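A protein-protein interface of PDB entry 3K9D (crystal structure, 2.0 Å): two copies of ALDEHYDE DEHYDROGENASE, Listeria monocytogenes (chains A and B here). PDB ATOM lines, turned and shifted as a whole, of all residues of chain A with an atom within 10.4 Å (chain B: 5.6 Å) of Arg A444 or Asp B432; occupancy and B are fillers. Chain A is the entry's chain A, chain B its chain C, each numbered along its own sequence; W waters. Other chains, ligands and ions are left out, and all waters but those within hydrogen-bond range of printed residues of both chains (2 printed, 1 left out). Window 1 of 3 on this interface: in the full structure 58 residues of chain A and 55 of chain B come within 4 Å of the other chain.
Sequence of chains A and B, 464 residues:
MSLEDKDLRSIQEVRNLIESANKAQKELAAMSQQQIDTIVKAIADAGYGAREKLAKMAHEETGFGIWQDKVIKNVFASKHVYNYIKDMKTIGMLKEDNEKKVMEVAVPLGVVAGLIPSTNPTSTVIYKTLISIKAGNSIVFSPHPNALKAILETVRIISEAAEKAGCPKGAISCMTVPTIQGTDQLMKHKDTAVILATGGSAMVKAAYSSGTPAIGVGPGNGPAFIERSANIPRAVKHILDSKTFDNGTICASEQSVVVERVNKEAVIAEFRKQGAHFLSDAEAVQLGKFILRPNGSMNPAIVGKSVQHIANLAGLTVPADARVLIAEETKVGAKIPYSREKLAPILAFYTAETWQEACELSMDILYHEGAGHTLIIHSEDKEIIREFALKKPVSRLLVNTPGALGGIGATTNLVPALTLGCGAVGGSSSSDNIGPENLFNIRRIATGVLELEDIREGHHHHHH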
ATOM      1  N   GLY A  92     -31.181  22.387 -23.081  1.00  0.00           N
ATOM      2  CA  GLY A  92     -30.375  23.613 -23.006  1.00  0.00           C
ATOM      3  C   GLY A  92     -30.323  24.207 -21.611  1.00  0.00           C
ATOM      4  O   GLY A  92     -30.461  23.486 -20.631  1.00  0.00           O
ATOM      5  N   MET A  93     -30.142  25.526 -21.538  1.00  0.00           N
ATOM      6  CA  MET A  93     -30.001  26.237 -20.268  1.00  0.00           C
ATOM      7  C   MET A  93     -31.276  26.162 -19.433  1.00  0.00           C
ATOM      8  O   MET A  93     -32.330  26.635 -19.862  1.00  0.00           O
ATOM      9  CB  MET A  93     -29.644  27.699 -20.511  1.00  0.00           C
ATOM     10  CG  MET A  93     -29.441  28.509 -19.244  1.00  0.00           C
ATOM     11  SD  MET A  93     -27.771  28.330 -18.597  1.00  0.00           S
ATOM     12  CE  MET A  93     -26.874  29.244 -19.837  1.00  0.00           C
ATOM     13  N   LEU A  94     -31.162  25.580 -18.241  1.00  0.00           N
ATOM     14  CA  LEU A  94     -32.302  25.417 -17.358  1.00  0.00           C
ATOM     15  C   LEU A  94     -32.349  26.492 -16.282  1.00  0.00           C
ATOM     16  O   LEU A  94     -33.409  27.046 -15.995  1.00  0.00           O
ATOM     17  CB  LEU A  94     -32.292  24.024 -16.714  1.00  0.00           C
ATOM     18  CG  LEU A  94     -32.311  22.773 -17.600  1.00  0.00           C
ATOM     19  CD1 LEU A  94     -32.161  21.533 -16.736  1.00  0.00           C
ATOM     20  CD2 LEU A  94     -33.584  22.681 -18.440  1.00  0.00           C
ATOM     21  N   LYS A  95     -31.198  26.783 -15.688  1.00  0.00           N
ATOM     22  CA  LYS A  95     -31.140  27.610 -14.494  1.00  0.00           C
ATOM     23  C   LYS A  95     -29.920  28.504 -14.551  1.00  0.00           C
ATOM     24  O   LYS A  95     -28.876  28.079 -15.042  1.00  0.00           O
ATOM     25  CB  LYS A  95     -31.035  26.720 -13.261  1.00  0.00           C
ATOM     26  CG  LYS A  95     -32.315  26.529 -12.490  1.00  0.00           C
ATOM     27  CD  LYS A  95     -32.133  25.510 -11.370  1.00  0.00           C
ATOM     28  CE  LYS A  95     -30.993  25.885 -10.424  1.00  0.00           C
ATOM     29  NZ  LYS A  95     -30.914  24.938  -9.268  1.00  0.00           N
ATOM     30  N   GLU A  96     -30.069  29.738 -14.067  1.00  0.00           N
ATOM     31  CA  GLU A  96     -28.975  30.693 -13.946  1.00  0.00           C
ATOM     32  C   GLU A  96     -29.031  31.310 -12.551  1.00  0.00           C
ATOM     33  O   GLU A  96     -29.690  32.336 -12.346  1.00  0.00           O
ATOM     34  CB  GLU A  96     -29.087  31.799 -15.009  1.00  0.00           C
ATOM     35  CG  GLU A  96     -28.840  31.344 -16.439  1.00  0.00           C
ATOM     36  CD  GLU A  96     -29.403  32.307 -17.464  1.00  0.00           C
ATOM     37  OE1 GLU A  96     -28.907  33.460 -17.548  1.00  0.00           O
ATOM     38  OE2 GLU A  96     -30.341  31.905 -18.189  1.00  0.00           O
ATOM     39  N   ASP A  97     -28.364  30.672 -11.591  1.00  0.00           N
ATOM     40  CA  ASP A  97     -28.295  31.197 -10.225  1.00  0.00           C
ATOM     41  C   ASP A  97     -27.187  32.237 -10.143  1.00  0.00           C
ATOM     42  O   ASP A  97     -26.006  31.895 -10.186  1.00  0.00           O
ATOM     43  CB  ASP A  97     -28.086  30.057  -9.207  1.00  0.00           C
ATOM     44  CG  ASP A  97     -28.108  30.534  -7.760  1.00  0.00           C
ATOM     45  OD1 ASP A  97     -28.398  29.699  -6.873  1.00  0.00           O
ATOM     46  OD2 ASP A  97     -27.834  31.727  -7.493  1.00  0.00           O
ATOM     47  N   LYS A 100     -25.303  32.246  -6.307  1.00  0.00           N
ATOM     48  CA  LYS A 100     -24.272  31.218  -6.196  1.00  0.00           C
ATOM     49  C   LYS A 100     -23.252  31.276  -7.345  1.00  0.00           C
ATOM     50  O   LYS A 100     -22.156  30.703  -7.236  1.00  0.00           O
ATOM     51  CB  LYS A 100     -24.915  29.835  -6.121  1.00  0.00           C
ATOM     52  CG  LYS A 100     -25.389  29.458  -4.721  1.00  0.00           C
ATOM     53  CD  LYS A 100     -25.719  27.978  -4.629  1.00  0.00           C
ATOM     54  CE  LYS A 100     -25.759  27.492  -3.176  1.00  0.00           C
ATOM     55  NZ  LYS A 100     -26.969  27.952  -2.423  1.00  0.00           N
ATOM     56  N   LYS A 101     -23.625  31.980  -8.421  1.00  0.00           N
ATOM     57  CA  LYS A 101     -22.856  32.073  -9.672  1.00  0.00           C
ATOM     58  C   LYS A 101     -22.660  30.700 -10.306  1.00  0.00           C
ATOM     59  O   LYS A 101     -21.550  30.315 -10.671  1.00  0.00           O
ATOM     60  CB  LYS A 101     -21.541  32.835  -9.478  1.00  0.00           C
ATOM     61  CG  LYS A 101     -21.723  34.333  -9.452  1.00  0.00           C
ATOM     62  CD  LYS A 101     -20.425  35.046  -9.096  1.00  0.00           C
ATOM     63  CE  LYS A 101     -20.436  35.524  -7.647  1.00  0.00           C
ATOM     64  NZ  LYS A 101     -21.221  36.789  -7.480  1.00  0.00           N
ATOM     65  N   VAL A 102     -23.771  29.966 -10.406  1.00  0.00           N
ATOM     66  CA  VAL A 102     -23.812  28.620 -10.975  1.00  0.00           C
ATOM     67  C   VAL A 102     -24.977  28.533 -11.981  1.00  0.00           C
ATOM     68  O   VAL A 102     -26.131  28.776 -11.629  1.00  0.00           O
ATOM     69  CB  VAL A 102     -24.011  27.526  -9.883  1.00  0.00           C
ATOM     70  CG1 VAL A 102     -24.078  26.123 -10.511  1.00  0.00           C
ATOM     71  CG2 VAL A 102     -22.915  27.566  -8.825  1.00  0.00           C
ATOM     72  N   MET A 103     -24.658  28.188 -13.225  1.00  0.00           N
ATOM     73  CA  MET A 103     -25.663  27.945 -14.254  1.00  0.00           C
ATOM     74  C   MET A 103     -25.818  26.445 -14.443  1.00  0.00           C
ATOM     75  O   MET A 103     -24.863  25.695 -14.223  1.00  0.00           O
ATOM     76  CB  MET A 103     -25.240  28.588 -15.581  1.00  0.00           C
ATOM     77  CG  MET A 103     -24.825  30.054 -15.467  1.00  0.00           C
ATOM     78  SD  MET A 103     -24.768  30.911 -17.056  1.00  0.00           S
ATOM     79  CE  MET A 103     -23.312  30.207 -17.825  1.00  0.00           C
ATOM     80  N   GLU A 104     -27.011  26.009 -14.843  1.00  0.00           N
ATOM     81  CA  GLU A 104     -27.281  24.588 -15.107  1.00  0.00           C
ATOM     82  C   GLU A 104     -27.818  24.383 -16.522  1.00  0.00           C
ATOM     83  O   GLU A 104     -28.702  25.117 -16.978  1.00  0.00           O
ATOM     84  CB  GLU A 104     -28.261  23.994 -14.078  1.00  0.00           C
ATOM     85  CG  GLU A 104     -27.774  24.046 -12.646  1.00  0.00           C
ATOM     86  CD  GLU A 104     -28.644  23.276 -11.671  1.00  0.00           C
ATOM     87  OE1 GLU A 104     -29.438  22.403 -12.093  1.00  0.00           O
ATOM     88  OE2 GLU A 104     -28.517  23.540 -10.457  1.00  0.00           O
ATOM     89  N   VAL A 105     -27.272  23.376 -17.203  1.00  0.00           N
ATOM     90  CA  VAL A 105     -27.573  23.070 -18.602  1.00  0.00           C
ATOM     91  C   VAL A 105     -27.878  21.581 -18.699  1.00  0.00           C
ATOM     92  O   VAL A 105     -27.096  20.752 -18.231  1.00  0.00           O
ATOM     93  CB  VAL A 105     -26.359  23.415 -19.548  1.00  0.00           C
ATOM     94  CG1 VAL A 105     -26.581  22.905 -20.995  1.00  0.00           C
ATOM     95  CG2 VAL A 105     -26.076  24.911 -19.567  1.00  0.00           C
ATOM     96  N   ALA A 106     -29.022  21.249 -19.301  1.00  0.00           N
ATOM     97  CA  ALA A 106     -29.394  19.871 -19.570  1.00  0.00           C
ATOM     98  C   ALA A 106     -28.536  19.270 -20.687  1.00  0.00           C
ATOM     99  O   ALA A 106     -28.363  19.863 -21.765  1.00  0.00           O
ATOM    100  CB  ALA A 106     -30.865  19.799 -19.926  1.00  0.00           C
ATOM    101  N   VAL A 107     -27.987  18.094 -20.417  1.00  0.00           N
ATOM    102  CA  VAL A 107     -27.183  17.374 -21.394  1.00  0.00           C
ATOM    103  C   VAL A 107     -27.843  16.037 -21.650  1.00  0.00           C
ATOM    104  O   VAL A 107     -27.941  15.230 -20.727  1.00  0.00           O
ATOM    105  CB  VAL A 107     -25.741  17.124 -20.874  1.00  0.00           C
ATOM    106  CG1 VAL A 107     -24.929  16.362 -21.895  1.00  0.00           C
ATOM    107  CG2 VAL A 107     -25.060  18.425 -20.566  1.00  0.00           C
ATOM    108  N   LEU A 109     -28.443  12.210 -22.578  1.00  0.00           N
ATOM    109  CA  LEU A 109     -27.612  11.034 -22.332  1.00  0.00           C
ATOM    110  C   LEU A 109     -26.945  10.550 -23.628  1.00  0.00           C
ATOM    111  O   LEU A 109     -25.763  10.211 -23.624  1.00  0.00           O
ATOM    112  CB  LEU A 109     -28.411   9.908 -21.627  1.00  0.00           C
ATOM    113  CG  LEU A 109     -28.349   9.725 -20.099  1.00  0.00           C
ATOM    114  CD1 LEU A 109     -28.180  11.048 -19.333  1.00  0.00           C
ATOM    115  CD2 LEU A 109     -29.499   8.870 -19.499  1.00  0.00           C
ATOM    116  N   GLU A 437     -36.510  13.548 -16.728  1.00  0.00           N
ATOM    117  CA  GLU A 437     -35.511  13.933 -15.733  1.00  0.00           C
ATOM    118  C   GLU A 437     -34.547  12.819 -15.316  1.00  0.00           C
ATOM    119  O   GLU A 437     -33.586  13.073 -14.591  1.00  0.00           O
ATOM    120  CB  GLU A 437     -36.203  14.549 -14.506  1.00  0.00           C
ATOM    121  CG  GLU A 437     -36.779  15.943 -14.765  1.00  0.00           C
ATOM    122  CD  GLU A 437     -37.422  16.581 -13.543  1.00  0.00           C
ATOM    123  OE1 GLU A 437     -38.190  17.546 -13.725  1.00  0.00           O
ATOM    124  OE2 GLU A 437     -37.168  16.134 -12.401  1.00  0.00           O
ATOM    125  N   PHE A 440     -31.559  12.962 -18.807  1.00  0.00           N
ATOM    126  CA  PHE A 440     -30.514  13.953 -19.070  1.00  0.00           C
ATOM    127  C   PHE A 440     -29.628  14.132 -17.846  1.00  0.00           C
ATOM    128  O   PHE A 440     -30.081  13.933 -16.710  1.00  0.00           O
ATOM    129  CB  PHE A 440     -31.041  15.295 -19.647  1.00  0.00           C
ATOM    130  CG  PHE A 440     -31.914  16.094 -18.717  1.00  0.00           C
ATOM    131  CD1 PHE A 440     -31.362  17.020 -17.838  1.00  0.00           C
ATOM    132  CD2 PHE A 440     -33.296  15.959 -18.759  1.00  0.00           C
ATOM    133  CE1 PHE A 440     -32.175  17.772 -16.988  1.00  0.00           C
ATOM    134  CE2 PHE A 440     -34.119  16.709 -17.921  1.00  0.00           C
ATOM    135  CZ  PHE A 440     -33.562  17.610 -17.028  1.00  0.00           C
ATOM    136  N   ASN A 441     -28.360  14.469 -18.102  1.00  0.00           N
ATOM    137  CA  ASN A 441     -27.418  14.882 -17.075  1.00  0.00           C
ATOM    138  C   ASN A 441     -27.496  16.398 -16.933  1.00  0.00           C
ATOM    139  O   ASN A 441     -27.838  17.095 -17.880  1.00  0.00           O
ATOM    140  CB  ASN A 441     -25.975  14.523 -17.466  1.00  0.00           C
ATOM    141  CG  ASN A 441     -25.691  13.038 -17.459  1.00  0.00           C
ATOM    142  OD1 ASN A 441     -25.073  12.533 -18.397  1.00  0.00           O
ATOM    143  ND2 ASN A 441     -26.088  12.332 -16.390  1.00  0.00           N
ATOM    144  N   ILE A 442     -27.152  16.909 -15.757  1.00  0.00           N
ATOM    145  CA  ILE A 442     -26.999  18.346 -15.579  1.00  0.00           C
ATOM    146  C   ILE A 442     -25.517  18.757 -15.603  1.00  0.00           C
ATOM    147  O   ILE A 442     -24.714  18.275 -14.799  1.00  0.00           O
ATOM    148  CB  ILE A 442     -27.700  18.828 -14.301  1.00  0.00           C
ATOM    149  CG1 ILE A 442     -29.212  18.526 -14.403  1.00  0.00           C
ATOM    150  CG2 ILE A 442     -27.397  20.299 -14.023  1.00  0.00           C
ATOM    151  CD1 ILE A 442     -30.134  19.578 -13.826  1.00  0.00           C
ATOM    152  N   ARG A 443     -25.171  19.627 -16.543  1.00  0.00           N
ATOM    153  CA  ARG A 443     -23.868  20.307 -16.547  1.00  0.00           C
ATOM    154  C   ARG A 443     -23.948  21.609 -15.745  1.00  0.00           C
ATOM    155  O   ARG A 443     -24.819  22.445 -15.993  1.00  0.00           O
ATOM    156  CB  ARG A 443     -23.413  20.594 -17.977  1.00  0.00           C
ATOM    157  CG  ARG A 443     -22.221  21.545 -18.114  1.00  0.00           C
ATOM    158  CD  ARG A 443     -22.024  21.988 -19.563  1.00  0.00           C
ATOM    159  NE  ARG A 443     -22.006  20.849 -20.484  1.00  0.00           N
ATOM    160  CZ  ARG A 443     -22.568  20.834 -21.692  1.00  0.00           C
ATOM    161  NH1 ARG A 443     -23.226  21.893 -22.145  1.00  0.00           N
ATOM    162  NH2 ARG A 443     -22.491  19.740 -22.439  1.00  0.00           N
ATOM    163  N   ARG A 444     -23.030  21.775 -14.799  1.00  0.00           N
ATOM    164  CA  ARG A 444     -22.956  22.993 -14.006  1.00  0.00           C
ATOM    165  C   ARG A 444     -21.760  23.859 -14.338  1.00  0.00           C
ATOM    166  O   ARG A 444     -20.622  23.383 -14.415  1.00  0.00           O
ATOM    167  CB  ARG A 444     -22.992  22.675 -12.520  1.00  0.00           C
ATOM    168  CG  ARG A 444     -24.330  22.118 -12.092  1.00  0.00           C
ATOM    169  CD  ARG A 444     -24.134  21.108 -11.032  1.00  0.00           C
ATOM    170  NE  ARG A 444     -25.363  20.411 -10.666  1.00  0.00           N
ATOM    171  CZ  ARG A 444     -25.621  19.148 -10.979  1.00  0.00           C
ATOM    172  NH1 ARG A 444     -24.755  18.443 -11.705  1.00  0.00           N
ATOM    173  NH2 ARG A 444     -26.749  18.586 -10.563  1.00  0.00           N
ATOM    174  N   ILE A 445     -22.033  25.141 -14.545  1.00  0.00           N
ATOM    175  CA  ILE A 445     -21.010  26.096 -14.941  1.00  0.00           C
ATOM    176  C   ILE A 445     -20.889  27.054 -13.778  1.00  0.00           C
ATOM    177  O   ILE A 445     -21.844  27.761 -13.458  1.00  0.00           O
ATOM    178  CB  ILE A 445     -21.382  26.843 -16.255  1.00  0.00           C
ATOM    179  CG1 ILE A 445     -21.630  25.839 -17.377  1.00  0.00           C
ATOM    180  CG2 ILE A 445     -20.289  27.851 -16.652  1.00  0.00           C
ATOM    181  CD1 ILE A 445     -23.074  25.363 -17.502  1.00  0.00           C
ATOM    182  N   ALA A 446     -19.724  27.041 -13.133  1.00  0.00           N
ATOM    183  CA  ALA A 446     -19.535  27.742 -11.869  1.00  0.00           C
ATOM    184  C   ALA A 446     -18.342  28.679 -11.894  1.00  0.00           C
ATOM    185  O   ALA A 446     -17.268  28.305 -12.372  1.00  0.00           O
ATOM    186  CB  ALA A 446     -19.391  26.747 -10.739  1.00  0.00           C
ATOM    187  N   THR A 447     -18.559  29.884 -11.360  1.00  0.00           N
ATOM    188  CA  THR A 447     -17.561  30.948 -11.257  1.00  0.00           C
ATOM    189  C   THR A 447     -16.904  30.952  -9.881  1.00  0.00           C
ATOM    190  O   THR A 447     -17.591  30.794  -8.872  1.00  0.00           O
ATOM    191  CB  THR A 447     -18.227  32.329 -11.514  1.00  0.00           C
ATOM    192  OG1 THR A 447     -18.893  32.301 -12.783  1.00  0.00           O
ATOM    193  CG2 THR A 447     -17.213  33.472 -11.507  1.00  0.00           C
ATOM    194  N   GLY A 448     -15.579  31.145  -9.854  1.00  0.00           N
ATOM    195  CA  GLY A 448     -14.825  31.268  -8.612  1.00  0.00           C
ATOM    196  C   GLY A 448     -15.327  32.356  -7.688  1.00  0.00           C
ATOM    197  O   GLY A 448     -15.574  33.485  -8.115  1.00  0.00           O
ATOM    198  N   SER B 395     -19.186  18.042 -17.476  1.00  0.00           N
ATOM    199  CA  SER B 395     -20.252  18.124 -16.469  1.00  0.00           C
ATOM    200  C   SER B 395     -20.028  19.283 -15.522  1.00  0.00           C
ATOM    201  O   SER B 395     -20.972  19.779 -14.897  1.00  0.00           O
ATOM    202  CB  SER B 395     -20.362  16.833 -15.684  1.00  0.00           C
ATOM    203  OG  SER B 395     -20.627  15.758 -16.565  1.00  0.00           O
ATOM    204  N   ARG B 396     -18.771  19.712 -15.424  1.00  0.00           N
ATOM    205  CA  ARG B 396     -18.428  20.900 -14.656  1.00  0.00           C
ATOM    206  C   ARG B 396     -17.538  21.842 -15.473  1.00  0.00           C
ATOM    207  O   ARG B 396     -16.429  21.471 -15.886  1.00  0.00           O
ATOM    208  CB  ARG B 396     -17.791  20.520 -13.313  1.00  0.00           C
ATOM    209  CG  ARG B 396     -16.605  19.583 -13.430  1.00  0.00           C
ATOM    210  CD  ARG B 396     -16.321  18.815 -12.158  1.00  0.00           C
ATOM    211  NE  ARG B 396     -17.470  18.045 -11.689  1.00  0.00           N
ATOM    212  CZ  ARG B 396     -17.892  16.886 -12.192  1.00  0.00           C
ATOM    213  NH1 ARG B 396     -17.285  16.304 -13.215  1.00  0.00           N
ATOM    214  NH2 ARG B 396     -18.940  16.296 -11.650  1.00  0.00           N
ATOM    215  N   LEU B 397     -18.036  23.049 -15.724  1.00  0.00           N
ATOM    216  CA  LEU B 397     -17.298  24.030 -16.495  1.00  0.00           C
ATOM    217  C   LEU B 397     -16.935  25.180 -15.575  1.00  0.00           C
ATOM    218  O   LEU B 397     -17.808  25.888 -15.059  1.00  0.00           O
ATOM    219  CB  LEU B 397     -18.101  24.517 -17.706  1.00  0.00           C
ATOM    220  CG  LEU B 397     -17.340  25.281 -18.793  1.00  0.00           C
ATOM    221  CD1 LEU B 397     -18.087  25.157 -20.086  1.00  0.00           C
ATOM    222  CD2 LEU B 397     -17.127  26.750 -18.466  1.00  0.00           C
ATOM    223  N   LEU B 398     -15.634  25.377 -15.388  1.00  0.00           N
ATOM    224  CA  LEU B 398     -15.172  26.263 -14.338  1.00  0.00           C
ATOM    225  C   LEU B 398     -14.716  27.594 -14.892  1.00  0.00           C
ATOM    226  O   LEU B 398     -14.030  27.656 -15.902  1.00  0.00           O
ATOM    227  CB  LEU B 398     -14.097  25.580 -13.478  1.00  0.00           C
ATOM    228  CG  LEU B 398     -14.400  24.129 -13.074  1.00  0.00           C
ATOM    229  CD1 LEU B 398     -13.162  23.478 -12.542  1.00  0.00           C
ATOM    230  CD2 LEU B 398     -15.588  23.985 -12.098  1.00  0.00           C
ATOM    231  N   LEU B 414     -20.232  24.889  -6.314  1.00  0.00           N
ATOM    232  CA  LEU B 414     -20.591  23.520  -6.640  1.00  0.00           C
ATOM    233  C   LEU B 414     -20.694  22.727  -5.343  1.00  0.00           C
ATOM    234  O   LEU B 414     -20.155  23.137  -4.310  1.00  0.00           O
ATOM    235  CB  LEU B 414     -19.567  22.878  -7.570  1.00  0.00           C
ATOM    236  CG  LEU B 414     -19.375  23.473  -8.970  1.00  0.00           C
ATOM    237  CD1 LEU B 414     -18.296  22.678  -9.705  1.00  0.00           C
ATOM    238  CD2 LEU B 414     -20.697  23.512  -9.750  1.00  0.00           C
ATOM    239  N   THR B 419     -15.839  12.891  -5.355  1.00  0.00           N
ATOM    240  CA  THR B 419     -16.291  12.001  -6.436  1.00  0.00           C
ATOM    241  C   THR B 419     -17.021  12.888  -7.432  1.00  0.00           C
ATOM    242  O   THR B 419     -18.098  13.411  -7.137  1.00  0.00           O
ATOM    243  CB  THR B 419     -17.245  10.869  -5.928  1.00  0.00           C
ATOM    244  OG1 THR B 419     -16.629  10.159  -4.860  1.00  0.00           O
ATOM    245  CG2 THR B 419     -17.593   9.868  -7.032  1.00  0.00           C
ATOM    246  N   LEU B 420     -16.419  13.067  -8.604  1.00  0.00           N
ATOM    247  CA  LEU B 420     -16.933  13.991  -9.598  1.00  0.00           C
ATOM    248  C   LEU B 420     -17.429  13.168 -10.759  1.00  0.00           C
ATOM    249  O   LEU B 420     -16.644  12.686 -11.568  1.00  0.00           O
ATOM    250  CB  LEU B 420     -15.853  15.008 -10.028  1.00  0.00           C
ATOM    251  CG  LEU B 420     -15.107  15.769  -8.919  1.00  0.00           C
ATOM    252  CD1 LEU B 420     -14.028  16.735  -9.483  1.00  0.00           C
ATOM    253  CD2 LEU B 420     -16.061  16.505  -7.975  1.00  0.00           C
ATOM    254  N   GLY B 421     -18.745  12.981 -10.811  1.00  0.00           N
ATOM    255  CA  GLY B 421     -19.368  12.139 -11.814  1.00  0.00           C
ATOM    256  C   GLY B 421     -19.151  12.701 -13.203  1.00  0.00           C
ATOM    257  O   GLY B 421     -19.152  13.911 -13.394  1.00  0.00           O
ATOM    258  N   SER B 430     -24.108   9.283 -13.371  1.00  0.00           N
ATOM    259  CA  SER B 430     -24.352  10.624 -12.840  1.00  0.00           C
ATOM    260  C   SER B 430     -23.250  11.598 -13.195  1.00  0.00           C
ATOM    261  O   SER B 430     -22.088  11.208 -13.315  1.00  0.00           O
ATOM    262  CB  SER B 430     -24.504  10.612 -11.320  1.00  0.00           C
ATOM    263  OG  SER B 430     -24.802  11.922 -10.861  1.00  0.00           O
ATOM    264  N   SER B 431     -23.634  12.869 -13.322  1.00  0.00           N
ATOM    265  CA  SER B 431     -22.723  13.954 -13.674  1.00  0.00           C
ATOM    266  C   SER B 431     -22.535  14.889 -12.489  1.00  0.00           C
ATOM    267  O   SER B 431     -21.808  15.874 -12.584  1.00  0.00           O
ATOM    268  CB  SER B 431     -23.272  14.730 -14.863  1.00  0.00           C
ATOM    269  OG  SER B 431     -24.476  15.422 -14.543  1.00  0.00           O
ATOM    270  N   ASP B 432     -23.185  14.553 -11.370  1.00  0.00           N
ATOM    271  CA  ASP B 432     -23.188  15.377 -10.175  1.00  0.00           C
ATOM    272  C   ASP B 432     -21.852  15.317  -9.456  1.00  0.00           C
ATOM    273  O   ASP B 432     -21.104  14.343  -9.588  1.00  0.00           O
ATOM    274  CB  ASP B 432     -24.263  14.888  -9.197  1.00  0.00           C
ATOM    275  CG  ASP B 432     -25.660  14.983  -9.767  1.00  0.00           C
ATOM    276  OD1 ASP B 432     -25.844  15.632 -10.818  1.00  0.00           O
ATOM    277  OD2 ASP B 432     -26.566  14.411  -9.144  1.00  0.00           O
ATOM    278  N   ASN B 433     -21.566  16.362  -8.685  1.00  0.00           N
ATOM    279  CA  ASN B 433     -20.598  16.253  -7.607  1.00  0.00           C
ATOM    280  C   ASN B 433     -21.371  15.512  -6.531  1.00  0.00           C
ATOM    281  O   ASN B 433     -22.374  16.029  -6.025  1.00  0.00           O
ATOM    282  CB  ASN B 433     -20.192  17.621  -7.101  1.00  0.00           C
ATOM    283  CG  ASN B 433     -19.149  18.297  -7.981  1.00  0.00           C
ATOM    284  OD1 ASN B 433     -19.083  18.078  -9.187  1.00  0.00           O
ATOM    285  ND2 ASN B 433     -18.342  19.148  -7.368  1.00  0.00           N
ATOM    286  N   ILE B 434     -20.937  14.293  -6.224  1.00  0.00           N
ATOM    287  CA  ILE B 434     -21.752  13.370  -5.424  1.00  0.00           C
ATOM    288  C   ILE B 434     -21.931  13.832  -3.972  1.00  0.00           C
ATOM    289  O   ILE B 434     -20.978  14.269  -3.307  1.00  0.00           O
ATOM    290  CB  ILE B 434     -21.229  11.900  -5.516  1.00  0.00           C
ATOM    291  CG1 ILE B 434     -21.113  11.444  -6.982  1.00  0.00           C
ATOM    292  CG2 ILE B 434     -22.085  10.935  -4.688  1.00  0.00           C
ATOM    293  CD1 ILE B 434     -22.337  11.740  -7.873  1.00  0.00           C
ATOM    294  N   ASN B 438     -27.607  11.753  -3.816  1.00  0.00           N
ATOM    295  CA  ASN B 438     -27.298  10.648  -4.725  1.00  0.00           C
ATOM    296  C   ASN B 438     -27.346   9.285  -4.034  1.00  0.00           C
ATOM    297  O   ASN B 438     -27.305   8.232  -4.685  1.00  0.00           O
ATOM    298  CB  ASN B 438     -25.927  10.862  -5.371  1.00  0.00           C
ATOM    299  CG  ASN B 438     -25.831  12.177  -6.102  1.00  0.00           C
ATOM    300  OD1 ASN B 438     -25.306  13.162  -5.569  1.00  0.00           O
ATOM    301  ND2 ASN B 438     -26.353  12.215  -7.332  1.00  0.00           N
HETATM  302  O   HOH W   1     -26.452  13.003 -13.974  1.00  0.00           O
HETATM  303  O   HOH W   2     -27.347  15.241 -13.217  1.00  0.00           O
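NH2 of Arg A444 lies within salt-bridge range of OD1 of Asp B432 (3.1 Å). O of Arg A444 lies within hydrogen-bond range of N of Leu B397 (2.9 Å). The backbone carbonyl oxygen (O) of Ile A442 lies within hydrogen-bond range of the side-chain hydroxyl (OG) of Ser B431, 2.9 Å away. The backbone NH (N) of Ala A446 is in hydrogen-bond range of the backbone carbonyl oxygen (O) of Leu B397 (3.0 Å). N of Arg A444 lies within hydrogen-bond range of O of Ser B395 (2.9 Å).
Of the 14 printed residues of chain B, 7 touch a printed residue of chain A. Of the 25 printed residues of chain A, 6 touch a printed residue of chain B. Hydrophobic or aromatic side chains of chain A within 4 Å of the printed part of chain B: Ile A445 and Ala A446. Among the printed residues, 12 pairs touch across the chains. Among the printed residues, Asp or Glu carboxylates within 4 Å of a Lys or Arg side-chain nitrogen of the other chain: Arg A444 with Asp B432 (3.1 Å).
Val A102 touches none of the printed residues of chain B. Of the printed residues of chain B, Ala A446 touches Leu B397 (3.0 Å), Leu B398 (3.5 Å) and Leu B414 (3.6 Å). Of chain A, only Arg A443 (3.4 Å) and Arg A444 (2.9 Å) come within 4 Å of Ser B395. Of chain A, only Arg A444 (3.1 Å) comes within 4 Å of Asp B432. No residue of chain A comes within 4 Å of Asn B433. Ile B434 touches none of the printed residues of chain A. The nearest printed residue of chain B that does not touch Arg A444 is Ser B431 (4.01 Å). The nearest printed residue of chain B that does not touch Ala A446 is Arg B396 (6.1 Å).
CB of Asn A441 touches OG of Ser B431, at 3.4 Å. CA of Arg A443 touches O of Ser B395 (3.4 Å). O of Arg A444 touches CA of Arg B396, 3.3 Å away. Leu B414 touches Arg A444. CA of Ile A445 touches O of Leu B397, at 3.2 Å. Ala A446 touches Leu B398. Ala A446 touches Leu B414.
No position is printed for both chains. Of the 12 pairs that touch across the chains among the printed residues, none has its exchanged pair printed and touching as well.
The guanidinium group (NE) of Arg B396 is in hydrogen-bond range of the side-chain amide oxygen (OD1) of Asn B433, at 3.0 Å. O of Ser B431 sits at hydrogen-bond distance from NH2 of Arg B396. The backbone carbonyl oxygen of Val A105 is in hydrogen-bond range of the backbone NH of Arg A443 (2.8 Å). N of Gly B421 lies within hydrogen-bond range of O of Asp B432.
Water W1 lies within hydrogen-bond range of the side-chain amide nitrogen of Asn A441 (2.5 Å) and the backbone NH of Ser B431 (2.9 Å). Water W2 lies within hydrogen-bond range of OD1 of Asp B432 (2.9 Å), N of Ile A442 (3.0 Å) and OG of Ser B431 (3.2 Å).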
